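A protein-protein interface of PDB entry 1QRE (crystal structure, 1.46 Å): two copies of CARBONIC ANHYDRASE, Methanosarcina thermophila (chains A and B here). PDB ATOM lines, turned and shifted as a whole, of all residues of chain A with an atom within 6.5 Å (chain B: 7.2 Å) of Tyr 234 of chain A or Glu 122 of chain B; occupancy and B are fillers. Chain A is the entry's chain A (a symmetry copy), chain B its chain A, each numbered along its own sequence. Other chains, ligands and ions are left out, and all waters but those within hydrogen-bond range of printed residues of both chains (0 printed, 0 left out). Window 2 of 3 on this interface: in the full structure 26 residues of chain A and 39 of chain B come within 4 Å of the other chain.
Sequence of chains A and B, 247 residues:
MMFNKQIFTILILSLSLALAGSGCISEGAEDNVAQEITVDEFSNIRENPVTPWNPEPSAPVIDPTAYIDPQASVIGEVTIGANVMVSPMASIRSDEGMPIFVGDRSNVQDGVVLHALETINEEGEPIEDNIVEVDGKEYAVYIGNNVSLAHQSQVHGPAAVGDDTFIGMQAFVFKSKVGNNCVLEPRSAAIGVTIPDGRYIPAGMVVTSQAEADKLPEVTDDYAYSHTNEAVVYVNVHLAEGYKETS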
ATOM      1  N   ASN A 229     -24.910  -2.220 -16.765  1.00  0.00           N
ATOM      2  CA  ASN A 229     -24.034  -3.079 -15.959  1.00  0.00           C
ATOM      3  C   ASN A 229     -24.736  -4.303 -15.410  1.00  0.00           C
ATOM      4  O   ASN A 229     -24.139  -5.400 -15.466  1.00  0.00           O
ATOM      5  CB  ASN A 229     -23.327  -2.318 -14.842  1.00  0.00           C
ATOM      6  CG  ASN A 229     -22.134  -3.153 -14.366  1.00  0.00           C
ATOM      7  OD1 ASN A 229     -21.243  -3.328 -15.236  1.00  0.00           O
ATOM      8  ND2 ASN A 229     -22.125  -3.611 -13.139  1.00  0.00           N
ATOM      9  N   GLU A 230     -25.958  -4.154 -14.897  1.00  0.00           N
ATOM     10  CA  GLU A 230     -26.674  -5.308 -14.352  1.00  0.00           C
ATOM     11  C   GLU A 230     -26.939  -6.353 -15.433  1.00  0.00           C
ATOM     12  O   GLU A 230     -26.788  -7.552 -15.173  1.00  0.00           O
ATOM     13  CB  GLU A 230     -27.995  -4.847 -13.732  1.00  0.00           C
ATOM     14  CG  GLU A 230     -28.980  -4.301 -14.766  1.00  0.00           C
ATOM     15  CD  GLU A 230     -29.882  -3.216 -14.211  1.00  0.00           C
ATOM     16  OE1 GLU A 230     -29.671  -2.824 -13.037  1.00  0.00           O
ATOM     17  OE2 GLU A 230     -30.805  -2.751 -14.915  1.00  0.00           O
ATOM     18  N   ALA A 231     -27.247  -5.926 -16.645  1.00  0.00           N
ATOM     19  CA  ALA A 231     -27.466  -6.880 -17.737  1.00  0.00           C
ATOM     20  C   ALA A 231     -26.161  -7.552 -18.100  1.00  0.00           C
ATOM     21  O   ALA A 231     -26.092  -8.785 -18.340  1.00  0.00           O
ATOM     22  CB  ALA A 231     -28.032  -6.118 -18.939  1.00  0.00           C
ATOM     23  N   VAL A 232     -25.073  -6.793 -18.193  1.00  0.00           N
ATOM     24  CA  VAL A 232     -23.773  -7.330 -18.558  1.00  0.00           C
ATOM     25  C   VAL A 232     -23.270  -8.352 -17.531  1.00  0.00           C
ATOM     26  O   VAL A 232     -22.716  -9.426 -17.853  1.00  0.00           O
ATOM     27  CB  VAL A 232     -22.719  -6.205 -18.703  1.00  0.00           C
ATOM     28  CG1 VAL A 232     -21.336  -6.748 -18.972  1.00  0.00           C
ATOM     29  CG2 VAL A 232     -23.156  -5.247 -19.813  1.00  0.00           C
ATOM     30  N   VAL A 233     -23.484  -8.087 -16.238  1.00  0.00           N
ATOM     31  CA  VAL A 233     -23.063  -8.997 -15.173  1.00  0.00           C
ATOM     32  C   VAL A 233     -23.890 -10.278 -15.244  1.00  0.00           C
ATOM     33  O   VAL A 233     -23.349 -11.394 -15.200  1.00  0.00           O
ATOM     34  CB  VAL A 233     -23.222  -8.324 -13.801  1.00  0.00           C
ATOM     35  CG1 VAL A 233     -23.112  -9.305 -12.641  1.00  0.00           C
ATOM     36  CG2 VAL A 233     -22.094  -7.272 -13.666  1.00  0.00           C
ATOM     37  N   TYR A 234     -25.201 -10.155 -15.456  1.00  0.00           N
ATOM     38  CA  TYR A 234     -26.015 -11.364 -15.632  1.00  0.00           C
ATOM     39  C   TYR A 234     -25.518 -12.191 -16.810  1.00  0.00           C
ATOM     40  O   TYR A 234     -25.344 -13.427 -16.691  1.00  0.00           O
ATOM     41  CB  TYR A 234     -27.468 -10.972 -15.834  1.00  0.00           C
ATOM     42  CG  TYR A 234     -28.475 -12.096 -15.737  1.00  0.00           C
ATOM     43  CD1 TYR A 234     -29.083 -12.417 -14.521  1.00  0.00           C
ATOM     44  CD2 TYR A 234     -28.828 -12.790 -16.869  1.00  0.00           C
ATOM     45  CE1 TYR A 234     -30.020 -13.442 -14.470  1.00  0.00           C
ATOM     46  CE2 TYR A 234     -29.773 -13.817 -16.827  1.00  0.00           C
ATOM     47  CZ  TYR A 234     -30.362 -14.110 -15.620  1.00  0.00           C
ATOM     48  OH  TYR A 234     -31.321 -15.119 -15.534  1.00  0.00           O
ATOM     49  N   VAL A 235     -25.256 -11.556 -17.943  1.00  0.00           N
ATOM     50  CA  VAL A 235     -24.809 -12.306 -19.118  1.00  0.00           C
ATOM     51  C   VAL A 235     -23.484 -12.954 -18.835  1.00  0.00           C
ATOM     52  O   VAL A 235     -23.229 -14.135 -19.098  1.00  0.00           O
ATOM     53  CB  VAL A 235     -24.720 -11.321 -20.315  1.00  0.00           C
ATOM     54  CG1 VAL A 235     -23.914 -11.959 -21.443  1.00  0.00           C
ATOM     55  CG2 VAL A 235     -26.134 -10.975 -20.723  1.00  0.00           C
ATOM     56  N   ASN A 236     -22.507 -12.223 -18.292  1.00  0.00           N
ATOM     57  CA  ASN A 236     -21.177 -12.717 -18.046  1.00  0.00           C
ATOM     58  C   ASN A 236     -21.039 -13.802 -17.010  1.00  0.00           C
ATOM     59  O   ASN A 236     -20.199 -14.703 -17.036  1.00  0.00           O
ATOM     60  CB  ASN A 236     -20.161 -11.567 -17.806  1.00  0.00           C
ATOM     61  CG  ASN A 236     -19.757 -10.888 -19.113  1.00  0.00           C
ATOM     62  OD1 ASN A 236     -18.712 -11.305 -19.648  1.00  0.00           O
ATOM     63  ND2 ASN A 236     -20.556  -9.968 -19.567  1.00  0.00           N
ATOM     64  N   VAL A 237     -21.920 -13.753 -15.968  1.00  0.00           N
ATOM     65  CA  VAL A 237     -21.933 -14.842 -14.973  1.00  0.00           C
ATOM     66  C   VAL A 237     -22.440 -16.125 -15.656  1.00  0.00           C
ATOM     67  O   VAL A 237     -21.889 -17.198 -15.439  1.00  0.00           O
ATOM     68  CB  VAL A 237     -22.815 -14.448 -13.785  1.00  0.00           C
ATOM     69  CG1 VAL A 237     -23.205 -15.675 -12.966  1.00  0.00           C
ATOM     70  CG2 VAL A 237     -22.096 -13.397 -12.950  1.00  0.00           C
ATOM     71  N   HIS A 238     -23.427 -15.977 -16.532  1.00  0.00           N
ATOM     72  CA  HIS A 238     -23.889 -17.152 -17.297  1.00  0.00           C
ATOM     73  C   HIS A 238     -22.856 -17.617 -18.292  1.00  0.00           C
ATOM     74  O   HIS A 238     -22.690 -18.832 -18.463  1.00  0.00           O
ATOM     75  CB  HIS A 238     -25.222 -16.846 -17.982  1.00  0.00           C
ATOM     76  CG  HIS A 238     -26.356 -16.872 -16.980  1.00  0.00           C
ATOM     77  ND1 HIS A 238     -26.684 -15.818 -16.163  1.00  0.00           N
ATOM     78  CD2 HIS A 238     -27.180 -17.894 -16.663  1.00  0.00           C
ATOM     79  CE1 HIS A 238     -27.705 -16.211 -15.383  1.00  0.00           C
ATOM     80  NE2 HIS A 238     -28.034 -17.466 -15.669  1.00  0.00           N
ATOM     81  N   LEU A 239     -22.095 -16.737 -18.950  1.00  0.00           N
ATOM     82  CA  LEU A 239     -21.053 -17.168 -19.861  1.00  0.00           C
ATOM     83  C   LEU A 239     -19.963 -17.875 -19.087  1.00  0.00           C
ATOM     84  O   LEU A 239     -19.428 -18.898 -19.549  1.00  0.00           O
ATOM     85  CB  LEU A 239     -20.435 -15.967 -20.620  1.00  0.00           C
ATOM     86  CG  LEU A 239     -21.280 -15.407 -21.737  1.00  0.00           C
ATOM     87  CD1 LEU A 239     -20.683 -14.118 -22.330  1.00  0.00           C
ATOM     88  CD2 LEU A 239     -21.400 -16.434 -22.881  1.00  0.00           C
ATOM     89  N   PRO B  52     -28.620 -19.694 -21.411  1.00  0.00           N
ATOM     90  CA  PRO B  52     -30.066 -19.576 -21.510  1.00  0.00           C
ATOM     91  C   PRO B  52     -30.547 -18.991 -22.815  1.00  0.00           C
ATOM     92  O   PRO B  52     -31.746 -19.045 -23.161  1.00  0.00           O
ATOM     93  CB  PRO B  52     -30.527 -18.666 -20.350  1.00  0.00           C
ATOM     94  CG  PRO B  52     -29.355 -18.763 -19.410  1.00  0.00           C
ATOM     95  CD  PRO B  52     -28.102 -18.975 -20.251  1.00  0.00           C
ATOM     96  N   TRP B  53     -29.688 -18.383 -23.630  1.00  0.00           N
ATOM     97  CA  TRP B  53     -30.056 -17.793 -24.903  1.00  0.00           C
ATOM     98  C   TRP B  53     -29.405 -18.557 -26.055  1.00  0.00           C
ATOM     99  O   TRP B  53     -29.494 -18.134 -27.217  1.00  0.00           O
ATOM    100  CB  TRP B  53     -29.654 -16.312 -24.964  1.00  0.00           C
ATOM    101  CG  TRP B  53     -28.171 -16.101 -24.776  1.00  0.00           C
ATOM    102  CD1 TRP B  53     -27.189 -16.158 -25.730  1.00  0.00           C
ATOM    103  CD2 TRP B  53     -27.522 -15.822 -23.539  1.00  0.00           C
ATOM    104  NE1 TRP B  53     -25.969 -15.928 -25.144  1.00  0.00           N
ATOM    105  CE2 TRP B  53     -26.133 -15.707 -23.802  1.00  0.00           C
ATOM    106  CE3 TRP B  53     -27.979 -15.622 -22.227  1.00  0.00           C
ATOM    107  CZ2 TRP B  53     -25.212 -15.441 -22.791  1.00  0.00           C
ATOM    108  CZ3 TRP B  53     -27.063 -15.353 -21.230  1.00  0.00           C
ATOM    109  CH2 TRP B  53     -25.693 -15.262 -21.524  1.00  0.00           C
ATOM    110  N   GLU B 118     -26.704  -9.022 -26.392  1.00  0.00           N
ATOM    111  CA  GLU B 118     -27.648 -10.136 -26.504  1.00  0.00           C
ATOM    112  C   GLU B 118     -28.735  -9.878 -27.544  1.00  0.00           C
ATOM    113  O   GLU B 118     -29.343  -8.801 -27.631  1.00  0.00           O
ATOM    114  CB  GLU B 118     -28.236 -10.450 -25.112  1.00  0.00           C
ATOM    115  CG  GLU B 118     -28.784 -11.869 -24.992  1.00  0.00           C
ATOM    116  CD  GLU B 118     -29.329 -12.221 -23.626  1.00  0.00           C
ATOM    117  OE1 GLU B 118     -28.839 -11.733 -22.591  1.00  0.00           O
ATOM    118  OE2 GLU B 118     -30.277 -13.047 -23.538  1.00  0.00           O
ATOM    119  N   ILE B 120     -31.110 -12.411 -28.230  1.00  0.00           N
ATOM    120  CA  ILE B 120     -32.301 -13.209 -27.877  1.00  0.00           C
ATOM    121  C   ILE B 120     -32.313 -13.296 -26.359  1.00  0.00           C
ATOM    122  O   ILE B 120     -31.267 -13.602 -25.775  1.00  0.00           O
ATOM    123  CB  ILE B 120     -32.273 -14.560 -28.591  1.00  0.00           C
ATOM    124  CG1 ILE B 120     -33.619 -15.294 -28.523  1.00  0.00           C
ATOM    125  CG2 ILE B 120     -31.189 -15.490 -28.070  1.00  0.00           C
ATOM    126  CD1 ILE B 120     -34.364 -15.267 -29.845  1.00  0.00           C
ATOM    127  N   ASN B 121     -33.416 -12.929 -25.702  1.00  0.00           N
ATOM    128  CA  ASN B 121     -33.397 -12.985 -24.235  1.00  0.00           C
ATOM    129  C   ASN B 121     -33.629 -14.411 -23.748  1.00  0.00           C
ATOM    130  O   ASN B 121     -34.062 -15.301 -24.488  1.00  0.00           O
ATOM    131  CB  ASN B 121     -34.370 -12.007 -23.599  1.00  0.00           C
ATOM    132  CG  ASN B 121     -35.839 -12.279 -23.832  1.00  0.00           C
ATOM    133  OD1 ASN B 121     -36.252 -13.410 -24.105  1.00  0.00           O
ATOM    134  ND2 ASN B 121     -36.642 -11.222 -23.716  1.00  0.00           N
ATOM    135  N   GLU B 122     -33.472 -14.626 -22.445  1.00  0.00           N
ATOM    136  CA  GLU B 122     -33.655 -15.914 -21.791  1.00  0.00           C
ATOM    137  C   GLU B 122     -35.068 -16.479 -21.872  1.00  0.00           C
ATOM    138  O   GLU B 122     -35.295 -17.640 -21.516  1.00  0.00           O
ATOM    139  CB  GLU B 122     -33.190 -15.857 -20.332  1.00  0.00           C
ATOM    140  CG  GLU B 122     -34.072 -15.165 -19.323  1.00  0.00           C
ATOM    141  CD  GLU B 122     -33.887 -13.672 -19.179  1.00  0.00           C
ATOM    142  OE1 GLU B 122     -34.533 -12.941 -19.961  1.00  0.00           O
ATOM    143  OE2 GLU B 122     -33.127 -13.198 -18.302  1.00  0.00           O
ATOM    144  N   GLU B 123     -36.036 -15.717 -22.358  1.00  0.00           N
ATOM    145  CA  GLU B 123     -37.411 -16.107 -22.567  1.00  0.00           C
ATOM    146  C   GLU B 123     -37.667 -16.437 -24.038  1.00  0.00           C
ATOM    147  O   GLU B 123     -38.793 -16.490 -24.532  1.00  0.00           O
ATOM    148  CB  GLU B 123     -38.350 -14.985 -22.116  1.00  0.00           C
ATOM    149  CG  GLU B 123     -38.223 -14.597 -20.651  1.00  0.00           C
ATOM    150  CD  GLU B 123     -39.152 -13.461 -20.271  1.00  0.00           C
ATOM    151  OE1 GLU B 123     -39.092 -12.964 -19.126  1.00  0.00           O
ATOM    152  OE2 GLU B 123     -39.966 -13.033 -21.122  1.00  0.00           O
ATOM    153  N   GLY B 124     -36.585 -16.578 -24.802  1.00  0.00           N
ATOM    154  CA  GLY B 124     -36.577 -16.915 -26.204  1.00  0.00           C
ATOM    155  C   GLY B 124     -36.984 -15.823 -27.168  1.00  0.00           C
ATOM    156  O   GLY B 124     -37.134 -16.080 -28.372  1.00  0.00           O
ATOM    157  N   GLU B 125     -37.149 -14.592 -26.689  1.00  0.00           N
ATOM    158  CA  GLU B 125     -37.569 -13.487 -27.530  1.00  0.00           C
ATOM    159  C   GLU B 125     -36.386 -12.712 -28.098  1.00  0.00           C
ATOM    160  O   GLU B 125     -35.474 -12.284 -27.389  1.00  0.00           O
ATOM    161  CB  GLU B 125     -38.442 -12.523 -26.732  1.00  0.00           C
ATOM    162  N   ILE B 127     -34.313  -9.722 -29.354  1.00  0.00           N
ATOM    163  CA  ILE B 127     -34.213  -8.324 -28.937  1.00  0.00           C
ATOM    164  C   ILE B 127     -33.909  -7.535 -30.200  1.00  0.00           C
ATOM    165  O   ILE B 127     -32.764  -7.308 -30.604  1.00  0.00           O
ATOM    166  CB  ILE B 127     -33.098  -8.135 -27.890  1.00  0.00           C
ATOM    167  CG1 ILE B 127     -33.323  -9.094 -26.723  1.00  0.00           C
ATOM    168  CG2 ILE B 127     -33.033  -6.684 -27.435  1.00  0.00           C
ATOM    169  CD1 ILE B 127     -32.156  -9.281 -25.791  1.00  0.00           C
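ND1 of His 238 of chain A lies within hydrogen-bond range of O of Tyr 234 of chain A (2.8 Å). The side-chain carboxylate (OE2) of Glu 118 of chain B sits close to the backbone carbonyl oxygen (O) of Ile 120 of chain B (2.5 Å).
OE2 of Glu 122 of chain B touches CE2 of Tyr 234 of chain A (3.7 Å). Val 235 of chain A touches Trp 53 of chain B. Glu 118 of chain B touches Val 235 of chain A. Pro 52 of chain B touches His 238 of chain A. CH2 of Trp 53 of chain B touches CB of His 238 of chain A, at 3.9 Å. Leu 239 of chain A touches Trp 53 of chain B (CD2 to CZ2, 3.9 Å).
Tyr 234 of chain A touches one residue of chain B. Printed residues of chain A within 4 Å of Glu 122 of chain B: Tyr 234 (3.7 Å). Printed residues of chain B within 4 Å of Val 235 of chain A: Trp 53 and Glu 118. Of the printed residues of chain A, Pro 52 of chain B touches His 238. Ala 231 of chain A touches none of the printed residues of chain B. Gly 124 of chain B touches none of the printed residues of chain A. The nearest printed residue of chain A that does not touch Glu 122 of chain B is His 238 of chain A (6.9 Å). The nearest printed residue of chain B that does not touch Leu 239 of chain A is Pro 52 of chain B (6.5 Å).
Printed residues of chain B that touch a printed residue of chain A: Pro 52, Trp 53, Glu 118 and Glu 122. Printed residues of chain A that touch a printed residue of chain B: Tyr 234, Val 235, His 238 and Leu 239. Hydrophobic or aromatic side chains of chain A that line the printed part of chain B: Tyr 234, Val 235, His 238 and Leu 239. Among the printed residues, 6 pairs touch across the chains.
No position is printed for both chains.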
